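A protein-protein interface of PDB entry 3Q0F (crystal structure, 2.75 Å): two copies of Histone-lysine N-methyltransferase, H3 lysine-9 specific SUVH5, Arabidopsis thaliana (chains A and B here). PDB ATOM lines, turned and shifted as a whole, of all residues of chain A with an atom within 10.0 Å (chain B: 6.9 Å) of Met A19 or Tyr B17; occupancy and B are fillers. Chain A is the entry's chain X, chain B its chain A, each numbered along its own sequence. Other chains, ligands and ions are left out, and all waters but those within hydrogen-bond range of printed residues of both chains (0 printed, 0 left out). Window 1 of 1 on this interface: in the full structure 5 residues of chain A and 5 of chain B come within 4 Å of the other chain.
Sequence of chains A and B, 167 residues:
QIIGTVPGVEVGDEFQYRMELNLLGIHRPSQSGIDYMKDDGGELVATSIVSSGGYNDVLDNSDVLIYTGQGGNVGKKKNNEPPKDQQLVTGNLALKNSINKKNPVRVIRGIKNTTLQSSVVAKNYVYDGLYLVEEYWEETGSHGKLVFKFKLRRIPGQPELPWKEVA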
ATOM      1  N   PHE A  15     -18.665  16.118  -1.830  1.00  0.00           N
ATOM      2  CA  PHE A  15     -19.027  14.936  -2.597  1.00  0.00           C
ATOM      3  C   PHE A  15     -19.219  13.718  -1.708  1.00  0.00           C
ATOM      4  O   PHE A  15     -18.673  13.621  -0.612  1.00  0.00           O
ATOM      5  CB  PHE A  15     -17.954  14.649  -3.644  1.00  0.00           C
ATOM      6  CG  PHE A  15     -17.484  15.873  -4.367  1.00  0.00           C
ATOM      7  CD1 PHE A  15     -18.075  16.259  -5.559  1.00  0.00           C
ATOM      8  CD2 PHE A  15     -16.464  16.652  -3.844  1.00  0.00           C
ATOM      9  CE1 PHE A  15     -17.654  17.384  -6.221  1.00  0.00           C
ATOM     10  CE2 PHE A  15     -16.039  17.789  -4.504  1.00  0.00           C
ATOM     11  CZ  PHE A  15     -16.632  18.153  -5.691  1.00  0.00           C
ATOM     12  N   GLN A  16     -19.994  12.774  -2.207  1.00  0.00           N
ATOM     13  CA  GLN A  16     -20.321  11.591  -1.449  1.00  0.00           C
ATOM     14  C   GLN A  16     -19.410  10.428  -1.834  1.00  0.00           C
ATOM     15  O   GLN A  16     -19.143   9.551  -1.025  1.00  0.00           O
ATOM     16  CB  GLN A  16     -21.784  11.244  -1.708  1.00  0.00           C
ATOM     17  CG  GLN A  16     -22.341  10.145  -0.845  1.00  0.00           C
ATOM     18  CD  GLN A  16     -23.724   9.725  -1.291  1.00  0.00           C
ATOM     19  OE1 GLN A  16     -24.303   8.787  -0.744  1.00  0.00           O
ATOM     20  NE2 GLN A  16     -24.260  10.414  -2.296  1.00  0.00           N
ATOM     21  N   TYR A  17     -18.925  10.438  -3.068  1.00  0.00           N
ATOM     22  CA  TYR A  17     -18.214   9.295  -3.620  1.00  0.00           C
ATOM     23  C   TYR A  17     -16.952   9.637  -4.402  1.00  0.00           C
ATOM     24  O   TYR A  17     -16.885  10.644  -5.107  1.00  0.00           O
ATOM     25  CB  TYR A  17     -19.159   8.475  -4.498  1.00  0.00           C
ATOM     26  CG  TYR A  17     -20.267   7.846  -3.709  1.00  0.00           C
ATOM     27  CD1 TYR A  17     -19.983   6.941  -2.694  1.00  0.00           C
ATOM     28  CD2 TYR A  17     -21.593   8.164  -3.957  1.00  0.00           C
ATOM     29  CE1 TYR A  17     -20.986   6.364  -1.956  1.00  0.00           C
ATOM     30  CE2 TYR A  17     -22.611   7.587  -3.224  1.00  0.00           C
ATOM     31  CZ  TYR A  17     -22.302   6.688  -2.223  1.00  0.00           C
ATOM     32  OH  TYR A  17     -23.312   6.114  -1.482  1.00  0.00           O
ATOM     33  N   ARG A  18     -15.960   8.767  -4.289  1.00  0.00           N
ATOM     34  CA  ARG A  18     -14.711   8.940  -5.004  1.00  0.00           C
ATOM     35  C   ARG A  18     -14.890   9.050  -6.513  1.00  0.00           C
ATOM     36  O   ARG A  18     -14.014   9.564  -7.193  1.00  0.00           O
ATOM     37  CB  ARG A  18     -13.779   7.775  -4.696  1.00  0.00           C
ATOM     38  CG  ARG A  18     -13.135   7.873  -3.359  1.00  0.00           C
ATOM     39  CD  ARG A  18     -12.105   8.934  -3.377  1.00  0.00           C
ATOM     40  NE  ARG A  18     -11.023   8.599  -4.294  1.00  0.00           N
ATOM     41  CZ  ARG A  18      -9.953   7.916  -3.930  1.00  0.00           C
ATOM     42  NH1 ARG A  18      -9.849   7.503  -2.681  1.00  0.00           N
ATOM     43  NH2 ARG A  18      -8.997   7.643  -4.802  1.00  0.00           N
ATOM     44  N   MET A  19     -16.002   8.548  -7.037  1.00  0.00           N
ATOM     45  CA  MET A  19     -16.210   8.544  -8.484  1.00  0.00           C
ATOM     46  C   MET A  19     -16.827   9.844  -8.949  1.00  0.00           C
ATOM     47  O   MET A  19     -16.683  10.220 -10.112  1.00  0.00           O
ATOM     48  CB  MET A  19     -17.066   7.359  -8.944  1.00  0.00           C
ATOM     49  CG  MET A  19     -16.391   5.987  -8.783  1.00  0.00           C
ATOM     50  SD  MET A  19     -14.774   5.812  -9.594  1.00  0.00           S
ATOM     51  CE  MET A  19     -15.141   6.343 -11.260  1.00  0.00           C
ATOM     52  N   GLU A  20     -17.520  10.530  -8.050  1.00  0.00           N
ATOM     53  CA  GLU A  20     -17.963  11.880  -8.360  1.00  0.00           C
ATOM     54  C   GLU A  20     -16.745  12.719  -8.743  1.00  0.00           C
ATOM     55  O   GLU A  20     -16.787  13.497  -9.694  1.00  0.00           O
ATOM     56  CB  GLU A  20     -18.699  12.493  -7.173  1.00  0.00           C
ATOM     57  CG  GLU A  20     -20.149  12.043  -7.039  1.00  0.00           C
ATOM     58  CD  GLU A  20     -20.693  12.260  -5.638  1.00  0.00           C
ATOM     59  OE1 GLU A  20     -21.821  12.781  -5.486  1.00  0.00           O
ATOM     60  OE2 GLU A  20     -19.980  11.912  -4.679  1.00  0.00           O
ATOM     61  N   LEU A  21     -15.652  12.528  -8.010  1.00  0.00           N
ATOM     62  CA  LEU A  21     -14.409  13.251  -8.263  1.00  0.00           C
ATOM     63  C   LEU A  21     -13.853  12.913  -9.633  1.00  0.00           C
ATOM     64  O   LEU A  21     -13.228  13.742 -10.283  1.00  0.00           O
ATOM     65  CB  LEU A  21     -13.358  12.910  -7.208  1.00  0.00           C
ATOM     66  CG  LEU A  21     -13.800  12.968  -5.750  1.00  0.00           C
ATOM     67  CD1 LEU A  21     -12.646  12.625  -4.819  1.00  0.00           C
ATOM     68  CD2 LEU A  21     -14.370  14.332  -5.431  1.00  0.00           C
ATOM     69  N   ASN A  22     -14.070  11.677 -10.056  1.00  0.00           N
ATOM     70  CA  ASN A  22     -13.628  11.222 -11.356  1.00  0.00           C
ATOM     71  C   ASN A  22     -14.435  11.902 -12.459  1.00  0.00           C
ATOM     72  O   ASN A  22     -13.879  12.450 -13.413  1.00  0.00           O
ATOM     73  CB  ASN A  22     -13.758   9.700 -11.441  1.00  0.00           C
ATOM     74  CG  ASN A  22     -13.307   9.149 -12.782  1.00  0.00           C
ATOM     75  OD1 ASN A  22     -13.716   9.629 -13.840  1.00  0.00           O
ATOM     76  ND2 ASN A  22     -12.456   8.138 -12.744  1.00  0.00           N
ATOM     77  N   LEU A  23     -15.752  11.872 -12.304  1.00  0.00           N
ATOM     78  CA  LEU A  23     -16.669  12.460 -13.266  1.00  0.00           C
ATOM     79  C   LEU A  23     -16.421  13.940 -13.523  1.00  0.00           C
ATOM     80  O   LEU A  23     -16.784  14.459 -14.576  1.00  0.00           O
ATOM     81  CB  LEU A  23     -18.109  12.252 -12.796  1.00  0.00           C
ATOM     82  CG  LEU A  23     -18.856  11.109 -13.487  1.00  0.00           C
ATOM     83  CD1 LEU A  23     -17.888  10.208 -14.237  1.00  0.00           C
ATOM     84  CD2 LEU A  23     -19.694  10.325 -12.490  1.00  0.00           C
ATOM     85  N   LEU A  24     -15.813  14.620 -12.559  1.00  0.00           N
ATOM     86  CA  LEU A  24     -15.547  16.043 -12.693  1.00  0.00           C
ATOM     87  C   LEU A  24     -14.081  16.301 -13.044  1.00  0.00           C
ATOM     88  O   LEU A  24     -13.676  17.433 -13.299  1.00  0.00           O
ATOM     89  CB  LEU A  24     -15.946  16.777 -11.420  1.00  0.00           C
ATOM     90  CG  LEU A  24     -17.436  16.677 -11.102  1.00  0.00           C
ATOM     91  CD1 LEU A  24     -17.763  17.382  -9.805  1.00  0.00           C
ATOM     92  CD2 LEU A  24     -18.251  17.252 -12.243  1.00  0.00           C
ATOM     93  N   GLY A  25     -13.287  15.240 -13.071  1.00  0.00           N
ATOM     94  CA  GLY A  25     -11.898  15.369 -13.458  1.00  0.00           C
ATOM     95  C   GLY A  25     -11.001  15.894 -12.357  1.00  0.00           C
ATOM     96  O   GLY A  25      -9.888  16.337 -12.614  1.00  0.00           O
ATOM     97  N   ILE A  26     -11.480  15.842 -11.121  1.00  0.00           N
ATOM     98  CA  ILE A  26     -10.684  16.268  -9.982  1.00  0.00           C
ATOM     99  C   ILE A  26      -9.669  15.199  -9.607  1.00  0.00           C
ATOM    100  O   ILE A  26      -8.515  15.490  -9.308  1.00  0.00           O
ATOM    101  CB  ILE A  26     -11.574  16.518  -8.774  1.00  0.00           C
ATOM    102  CG1 ILE A  26     -12.767  17.386  -9.168  1.00  0.00           C
ATOM    103  CG2 ILE A  26     -10.783  17.145  -7.643  1.00  0.00           C
ATOM    104  CD1 ILE A  26     -13.824  17.458  -8.088  1.00  0.00           C
ATOM    105  N   HIS A  27     -10.110  13.949  -9.627  1.00  0.00           N
ATOM    106  CA  HIS A  27      -9.270  12.840  -9.222  1.00  0.00           C
ATOM    107  C   HIS A  27      -9.787  11.592  -9.918  1.00  0.00           C
ATOM    108  O   HIS A  27     -10.959  11.251  -9.784  1.00  0.00           O
ATOM    109  CB  HIS A  27      -9.324  12.677  -7.699  1.00  0.00           C
ATOM    110  CG  HIS A  27      -8.180  11.901  -7.136  1.00  0.00           C
ATOM    111  ND1 HIS A  27      -8.312  10.616  -6.670  1.00  0.00           N
ATOM    112  CD2 HIS A  27      -6.875  12.222  -6.987  1.00  0.00           C
ATOM    113  CE1 HIS A  27      -7.142  10.179  -6.247  1.00  0.00           C
ATOM    114  NE2 HIS A  27      -6.251  11.134  -6.431  1.00  0.00           N
ATOM    115  N   ARG A  28      -8.924  10.919 -10.671  1.00  0.00           N
ATOM    116  CA  ARG A  28      -9.379   9.835 -11.536  1.00  0.00           C
ATOM    117  C   ARG A  28      -9.458   8.474 -10.856  1.00  0.00           C
ATOM    118  O   ARG A  28     -10.453   7.770 -10.997  1.00  0.00           O
ATOM    119  CB  ARG A  28      -8.531   9.752 -12.805  1.00  0.00           C
ATOM    120  CG  ARG A  28      -8.671  10.971 -13.704  1.00  0.00           C
ATOM    121  CD  ARG A  28      -7.854  10.827 -14.980  1.00  0.00           C
ATOM    122  NE  ARG A  28      -6.423  10.717 -14.710  1.00  0.00           N
ATOM    123  CZ  ARG A  28      -5.531  10.251 -15.580  1.00  0.00           C
ATOM    124  NH1 ARG A  28      -5.920   9.846 -16.784  1.00  0.00           N
ATOM    125  NH2 ARG A  28      -4.250  10.186 -15.244  1.00  0.00           N
ATOM    126  N   PRO A  29      -8.409   8.086 -10.123  1.00  0.00           N
ATOM    127  CA  PRO A  29      -8.487   6.743  -9.555  1.00  0.00           C
ATOM    128  C   PRO A  29      -9.669   6.596  -8.597  1.00  0.00           C
ATOM    129  O   PRO A  29     -10.097   7.557  -7.970  1.00  0.00           O
ATOM    130  CB  PRO A  29      -7.152   6.601  -8.819  1.00  0.00           C
ATOM    131  CG  PRO A  29      -6.251   7.546  -9.472  1.00  0.00           C
ATOM    132  CD  PRO A  29      -7.113   8.722  -9.849  1.00  0.00           C
ATOM    133  N   SER A  30     -10.194   5.384  -8.505  1.00  0.00           N
ATOM    134  CA  SER A  30     -11.361   5.096  -7.686  1.00  0.00           C
ATOM    135  C   SER A  30     -10.970   4.828  -6.234  1.00  0.00           C
ATOM    136  O   SER A  30     -11.793   4.946  -5.328  1.00  0.00           O
ATOM    137  CB  SER A  30     -12.093   3.889  -8.261  1.00  0.00           C
ATOM    138  OG  SER A  30     -11.196   2.812  -8.459  1.00  0.00           O
ATOM    139  N   GLN A  31      -9.709   4.471  -6.020  1.00  0.00           N
ATOM    140  CA  GLN A  31      -9.228   4.158  -4.685  1.00  0.00           C
ATOM    141  C   GLN A  31      -7.874   4.781  -4.392  1.00  0.00           C
ATOM    142  O   GLN A  31      -7.661   5.344  -3.325  1.00  0.00           O
ATOM    143  CB  GLN A  31      -9.143   2.650  -4.497  1.00  0.00           C
ATOM    144  CG  GLN A  31     -10.480   1.954  -4.615  1.00  0.00           C
ATOM    145  CD  GLN A  31     -10.417   0.516  -4.189  1.00  0.00           C
ATOM    146  OE1 GLN A  31     -11.225  -0.297  -4.618  1.00  0.00           O
ATOM    147  NE2 GLN A  31      -9.454   0.191  -3.339  1.00  0.00           N
ATOM    148  N   SER A  32      -6.955   4.671  -5.341  1.00  0.00           N
ATOM    149  CA  SER A  32      -5.611   5.180  -5.132  1.00  0.00           C
ATOM    150  C   SER A  32      -5.665   6.645  -4.704  1.00  0.00           C
ATOM    151  O   SER A  32      -6.361   7.453  -5.321  1.00  0.00           O
ATOM    152  CB  SER A  32      -4.780   5.013  -6.400  1.00  0.00           C
ATOM    153  OG  SER A  32      -3.445   5.449  -6.199  1.00  0.00           O
ATOM    154  N   VAL A  50      -6.010  12.433  -2.319  1.00  0.00           N
ATOM    155  CA  VAL A  50      -7.144  12.310  -1.427  1.00  0.00           C
ATOM    156  C   VAL A  50      -6.617  11.900  -0.066  1.00  0.00           C
ATOM    157  O   VAL A  50      -5.885  10.924   0.054  1.00  0.00           O
ATOM    158  CB  VAL A  50      -8.157  11.262  -1.926  1.00  0.00           C
ATOM    159  CG1 VAL A  50      -9.284  11.110  -0.928  1.00  0.00           C
ATOM    160  CG2 VAL A  50      -8.708  11.654  -3.286  1.00  0.00           C
ATOM    161  N   ILE A 108      -8.118  16.707  -1.711  1.00  0.00           N
ATOM    162  CA  ILE A 108      -9.452  16.370  -1.248  1.00  0.00           C
ATOM    163  C   ILE A 108      -9.310  15.726   0.110  1.00  0.00           C
ATOM    164  O   ILE A 108      -8.456  14.869   0.302  1.00  0.00           O
ATOM    165  CB  ILE A 108     -10.145  15.384  -2.196  1.00  0.00           C
ATOM    166  CG1 ILE A 108     -10.399  16.046  -3.544  1.00  0.00           C
ATOM    167  CG2 ILE A 108     -11.442  14.881  -1.608  1.00  0.00           C
ATOM    168  CD1 ILE A 108      -9.196  16.006  -4.445  1.00  0.00           C
ATOM    169  N   ASN A 124     -18.803  12.882   1.895  1.00  0.00           N
ATOM    170  CA  ASN A 124     -17.633  12.418   2.626  1.00  0.00           C
ATOM    171  C   ASN A 124     -16.332  13.038   2.164  1.00  0.00           C
ATOM    172  O   ASN A 124     -15.280  12.701   2.682  1.00  0.00           O
ATOM    173  CB  ASN A 124     -17.510  10.903   2.491  1.00  0.00           C
ATOM    174  CG  ASN A 124     -18.766  10.175   2.922  1.00  0.00           C
ATOM    175  OD1 ASN A 124     -19.589   9.774   2.083  1.00  0.00           O
ATOM    176  ND2 ASN A 124     -18.925   9.996   4.239  1.00  0.00           N
ATOM    177  N   TYR A 125     -16.397  13.923   1.177  1.00  0.00           N
ATOM    178  CA  TYR A 125     -15.189  14.508   0.593  1.00  0.00           C
ATOM    179  C   TYR A 125     -15.332  16.011   0.328  1.00  0.00           C
ATOM    180  O   TYR A 125     -16.355  16.468  -0.181  1.00  0.00           O
ATOM    181  CB  TYR A 125     -14.832  13.783  -0.711  1.00  0.00           C
ATOM    182  CG  TYR A 125     -14.558  12.312  -0.537  1.00  0.00           C
ATOM    183  CD1 TYR A 125     -13.349  11.870  -0.021  1.00  0.00           C
ATOM    184  CD2 TYR A 125     -15.509  11.363  -0.885  1.00  0.00           C
ATOM    185  CE1 TYR A 125     -13.096  10.523   0.151  1.00  0.00           C
ATOM    186  CE2 TYR A 125     -15.266  10.017  -0.717  1.00  0.00           C
ATOM    187  CZ  TYR A 125     -14.058   9.597  -0.196  1.00  0.00           C
ATOM    188  OH  TYR A 125     -13.801   8.248  -0.019  1.00  0.00           O
ATOM    189  N   PHE B  15     -24.891   3.606 -18.431  1.00  0.00           N
ATOM    190  CA  PHE B  15     -24.069   4.208 -17.393  1.00  0.00           C
ATOM    191  C   PHE B  15     -22.614   3.800 -17.523  1.00  0.00           C
ATOM    192  O   PHE B  15     -22.293   2.781 -18.110  1.00  0.00           O
ATOM    193  CB  PHE B  15     -24.596   3.820 -16.025  1.00  0.00           C
ATOM    194  CG  PHE B  15     -26.080   3.909 -15.917  1.00  0.00           C
ATOM    195  CD1 PHE B  15     -26.683   5.058 -15.457  1.00  0.00           C
ATOM    196  CD2 PHE B  15     -26.879   2.844 -16.293  1.00  0.00           C
ATOM    197  CE1 PHE B  15     -28.053   5.144 -15.361  1.00  0.00           C
ATOM    198  CE2 PHE B  15     -28.250   2.923 -16.204  1.00  0.00           C
ATOM    199  CZ  PHE B  15     -28.838   4.074 -15.735  1.00  0.00           C
ATOM    200  N   GLN B  16     -21.735   4.613 -16.962  1.00  0.00           N
ATOM    201  CA  GLN B  16     -20.308   4.397 -17.088  1.00  0.00           C
ATOM    202  C   GLN B  16     -19.763   3.721 -15.831  1.00  0.00           C
ATOM    203  O   GLN B  16     -18.763   3.009 -15.882  1.00  0.00           O
ATOM    204  CB  GLN B  16     -19.633   5.750 -17.296  1.00  0.00           C
ATOM    205  CG  GLN B  16     -18.161   5.694 -17.631  1.00  0.00           C
ATOM    206  CD  GLN B  16     -17.523   7.075 -17.645  1.00  0.00           C
ATOM    207  OE1 GLN B  16     -16.312   7.209 -17.831  1.00  0.00           O
ATOM    208  NE2 GLN B  16     -18.339   8.110 -17.441  1.00  0.00           N
ATOM    209  N   TYR B  17     -20.441   3.942 -14.706  1.00  0.00           N
ATOM    210  CA  TYR B  17     -19.920   3.552 -13.401  1.00  0.00           C
ATOM    211  C   TYR B  17     -20.939   2.907 -12.452  1.00  0.00           C
ATOM    212  O   TYR B  17     -22.115   3.275 -12.396  1.00  0.00           O
ATOM    213  CB  TYR B  17     -19.251   4.749 -12.711  1.00  0.00           C
ATOM    214  CG  TYR B  17     -18.024   5.217 -13.430  1.00  0.00           C
ATOM    215  CD1 TYR B  17     -16.947   4.366 -13.614  1.00  0.00           C
ATOM    216  CD2 TYR B  17     -17.944   6.499 -13.944  1.00  0.00           C
ATOM    217  CE1 TYR B  17     -15.821   4.775 -14.292  1.00  0.00           C
ATOM    218  CE2 TYR B  17     -16.818   6.921 -14.619  1.00  0.00           C
ATOM    219  CZ  TYR B  17     -15.760   6.050 -14.794  1.00  0.00           C
ATOM    220  OH  TYR B  17     -14.629   6.446 -15.463  1.00  0.00           O
ATOM    221  N   ARG B  18     -20.455   1.948 -11.681  1.00  0.00           N
ATOM    222  CA  ARG B  18     -21.296   1.258 -10.731  1.00  0.00           C
ATOM    223  C   ARG B  18     -21.934   2.204  -9.729  1.00  0.00           C
ATOM    224  O   ARG B  18     -22.956   1.878  -9.123  1.00  0.00           O
ATOM    225  CB  ARG B  18     -20.482   0.199  -9.996  1.00  0.00           C
ATOM    226  CG  ARG B  18     -20.251  -1.043 -10.815  1.00  0.00           C
ATOM    227  CD  ARG B  18     -21.544  -1.792 -10.930  1.00  0.00           C
ATOM    228  NE  ARG B  18     -21.982  -2.284  -9.625  1.00  0.00           N
ATOM    229  CZ  ARG B  18     -21.576  -3.437  -9.111  1.00  0.00           C
ATOM    230  NH1 ARG B  18     -20.725  -4.184  -9.800  1.00  0.00           N
ATOM    231  NH2 ARG B  18     -22.006  -3.834  -7.919  1.00  0.00           N
ATOM    232  N   MET B  19     -21.330   3.370  -9.533  1.00  0.00           N
ATOM    233  CA  MET B  19     -21.854   4.302  -8.537  1.00  0.00           C
ATOM    234  C   MET B  19     -22.966   5.170  -9.101  1.00  0.00           C
ATOM    235  O   MET B  19     -23.820   5.646  -8.362  1.00  0.00           O
ATOM    236  CB  MET B  19     -20.740   5.160  -7.932  1.00  0.00           C
ATOM    237  CG  MET B  19     -19.721   4.372  -7.101  1.00  0.00           C
ATOM    238  SD  MET B  19     -20.398   3.411  -5.714  1.00  0.00           S
ATOM    239  CE  MET B  19     -21.429   4.617  -4.877  1.00  0.00           C
ATOM    240  N   GLU B  20     -22.961   5.378 -10.411  1.00  0.00           N
ATOM    241  CA  GLU B  20     -24.094   6.035 -11.040  1.00  0.00           C
ATOM    242  C   GLU B  20     -25.365   5.272 -10.674  1.00  0.00           C
ATOM    243  O   GLU B  20     -26.395   5.872 -10.362  1.00  0.00           O
ATOM    244  CB  GLU B  20     -23.923   6.102 -12.555  1.00  0.00           C
ATOM    245  CG  GLU B  20     -22.986   7.211 -13.026  1.00  0.00           C
ATOM    246  CD  GLU B  20     -22.442   6.970 -14.434  1.00  0.00           C
ATOM    247  OE1 GLU B  20     -22.450   7.911 -15.262  1.00  0.00           O
ATOM    248  OE2 GLU B  20     -22.009   5.831 -14.714  1.00  0.00           O
ATOM    249  N   LEU B  21     -25.277   3.944 -10.691  1.00  0.00           N
ATOM    250  CA  LEU B  21     -26.409   3.083 -10.367  1.00  0.00           C
ATOM    251  C   LEU B  21     -26.850   3.288  -8.932  1.00  0.00           C
ATOM    252  O   LEU B  21     -28.029   3.162  -8.608  1.00  0.00           O
ATOM    253  CB  LEU B  21     -26.034   1.612 -10.556  1.00  0.00           C
ATOM    254  CG  LEU B  21     -25.364   1.228 -11.874  1.00  0.00           C
ATOM    255  CD1 LEU B  21     -25.106  -0.268 -11.916  1.00  0.00           C
ATOM    256  CD2 LEU B  21     -26.212   1.671 -13.057  1.00  0.00           C
ATOM    257  N   ASN B  22     -25.882   3.576  -8.070  1.00  0.00           N
ATOM    258  CA  ASN B  22     -26.159   3.839  -6.671  1.00  0.00           C
ATOM    259  C   ASN B  22     -26.908   5.155  -6.506  1.00  0.00           C
ATOM    260  O   ASN B  22     -27.933   5.228  -5.820  1.00  0.00           O
ATOM    261  CB  ASN B  22     -24.852   3.870  -5.893  1.00  0.00           C
ATOM    262  CG  ASN B  22     -25.061   4.120  -4.425  1.00  0.00           C
ATOM    263  OD1 ASN B  22     -25.771   5.046  -4.036  1.00  0.00           O
ATOM    264  ND2 ASN B  22     -24.434   3.297  -3.592  1.00  0.00           N
ATOM    265  N   LYS B 123     -19.604   4.370 -21.425  1.00  0.00           N
ATOM    266  CA  LYS B 123     -20.789   3.681 -20.907  1.00  0.00           C
ATOM    267  C   LYS B 123     -20.618   2.145 -20.885  1.00  0.00           C
ATOM    268  O   LYS B 123     -20.489   1.508 -21.930  1.00  0.00           O
ATOM    269  CB  LYS B 123     -22.038   4.098 -21.696  1.00  0.00           C
ATOM    270  N   ASN B 124     -20.622   1.560 -19.686  1.00  0.00           N
ATOM    271  CA  ASN B 124     -20.353   0.131 -19.519  1.00  0.00           C
ATOM    272  C   ASN B 124     -21.508  -0.685 -18.940  1.00  0.00           C
ATOM    273  O   ASN B 124     -21.366  -1.888 -18.732  1.00  0.00           O
ATOM    274  CB  ASN B 124     -19.142  -0.071 -18.616  1.00  0.00           C
ATOM    275  CG  ASN B 124     -17.935   0.715 -19.067  1.00  0.00           C
ATOM    276  OD1 ASN B 124     -17.648   1.785 -18.529  1.00  0.00           O
ATOM    277  ND2 ASN B 124     -17.207   0.183 -20.047  1.00  0.00           N
ATOM    278  N   TYR B 125     -22.642  -0.040 -18.678  1.00  0.00           N
ATOM    279  CA  TYR B 125     -23.768  -0.708 -18.044  1.00  0.00           C
ATOM    280  C   TYR B 125     -25.094  -0.307 -18.666  1.00  0.00           C
ATOM    281  O   TYR B 125     -25.332   0.869 -18.923  1.00  0.00           O
ATOM    282  CB  TYR B 125     -23.790  -0.405 -16.537  1.00  0.00           C
ATOM    283  CG  TYR B 125     -22.543  -0.852 -15.822  1.00  0.00           C
ATOM    284  CD1 TYR B 125     -22.344  -2.192 -15.504  1.00  0.00           C
ATOM    285  CD2 TYR B 125     -21.545   0.058 -15.490  1.00  0.00           C
ATOM    286  CE1 TYR B 125     -21.192  -2.611 -14.867  1.00  0.00           C
ATOM    287  CE2 TYR B 125     -20.384  -0.352 -14.848  1.00  0.00           C
ATOM    288  CZ  TYR B 125     -20.214  -1.686 -14.538  1.00  0.00           C
ATOM    289  OH  TYR B 125     -19.064  -2.090 -13.896  1.00  0.00           O
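Tyr A17 touches Met B19, and with the chains exchanged Met A19 touches Tyr B17.
Tyr A17 touches Asn B22, and with the chains exchanged Asn A22 touches Tyr B17.
Of the 6 pairs that touch across the chains among the printed residues, 4 have their exchanged pair printed and touching as well.
The side-chain amide oxygen (OE1) of Gln B16 sits at hydrogen-bond distance from the side-chain hydroxyl (OH) of Tyr B17 (3.0 Å).
The side-chain amide nitrogen of Asn A22 lies within hydrogen-bond range of the backbone carbonyl oxygen of Arg A28 (2.7 Å).
OD1 of Asn B124 sits close to O of Gln B16 (3.1 Å).
OE2 of Glu B20 lies within hydrogen-bond range of N of Gln B16, 2.6 Å away.
The backbone NH of Asn A22 sits close to the backbone carbonyl oxygen of His A27.
The backbone NH of Tyr B17 sits at hydrogen-bond distance from the side-chain carboxylate of Glu B20 (2.5 Å).
Of the 22 printed residues of chain A, 4 touch a printed residue of chain B.
Hydrophobic or aromatic side chains of chain A that line the printed part of chain B: Tyr A17, Met A19 and Leu A23.
Along chain A the printed residues that touch a printed residue of chain B span positions 17 to 23.
Printed residues of chain B that touch a printed residue of chain A: Gln B16, Tyr B17, Met B19 and Asn B22.
Among the printed residues, no Asp or Glu carboxylate lies within 4 Å of a Lys or Arg side-chain nitrogen of the other chain.
Of chain B, only Tyr B17 (3.5 Å) comes within 4 Å of Met A19.
Tyr B17 touches just these residues of chain A: Met A19 (3.5 Å), Asn A22 (3.7 Å) and Leu A23 (3.5 Å).
Of the printed residues of chain A, Gln B16 touches Leu A23 (3.9 Å).
No residue of chain A comes within 4 Å of Glu B20.
Printed residues of chain B within 4 Å of Asn A22: Tyr B17.
Printed residues of chain B within 4 Å of Tyr A17: Met B19 and Asn B22.
Of the printed residues of chain A, Asn B22 touches Tyr A17 (3.7 Å).
Printed residues of chain B within 4 Å of Leu A23: Gln B16 and Tyr B17.
Printed residues of chain A within 4 Å of Met B19: Tyr A17.
Gly A25 touches none of the printed residues of chain B.
The nearest residue of chain B that does not touch Met A19 is Met B19 (4.1 Å).
Tyr A17 touches Met B19.
Asn B22 touches Tyr A17 (ND2 to OH, 3.7 Å).
CE of Met A19 touches CE1 of Tyr B17 (3.5 Å).
Tyr B17 touches Asn A22.
Leu A23 touches Gln B16.
Leu A23 touches Tyr B17.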
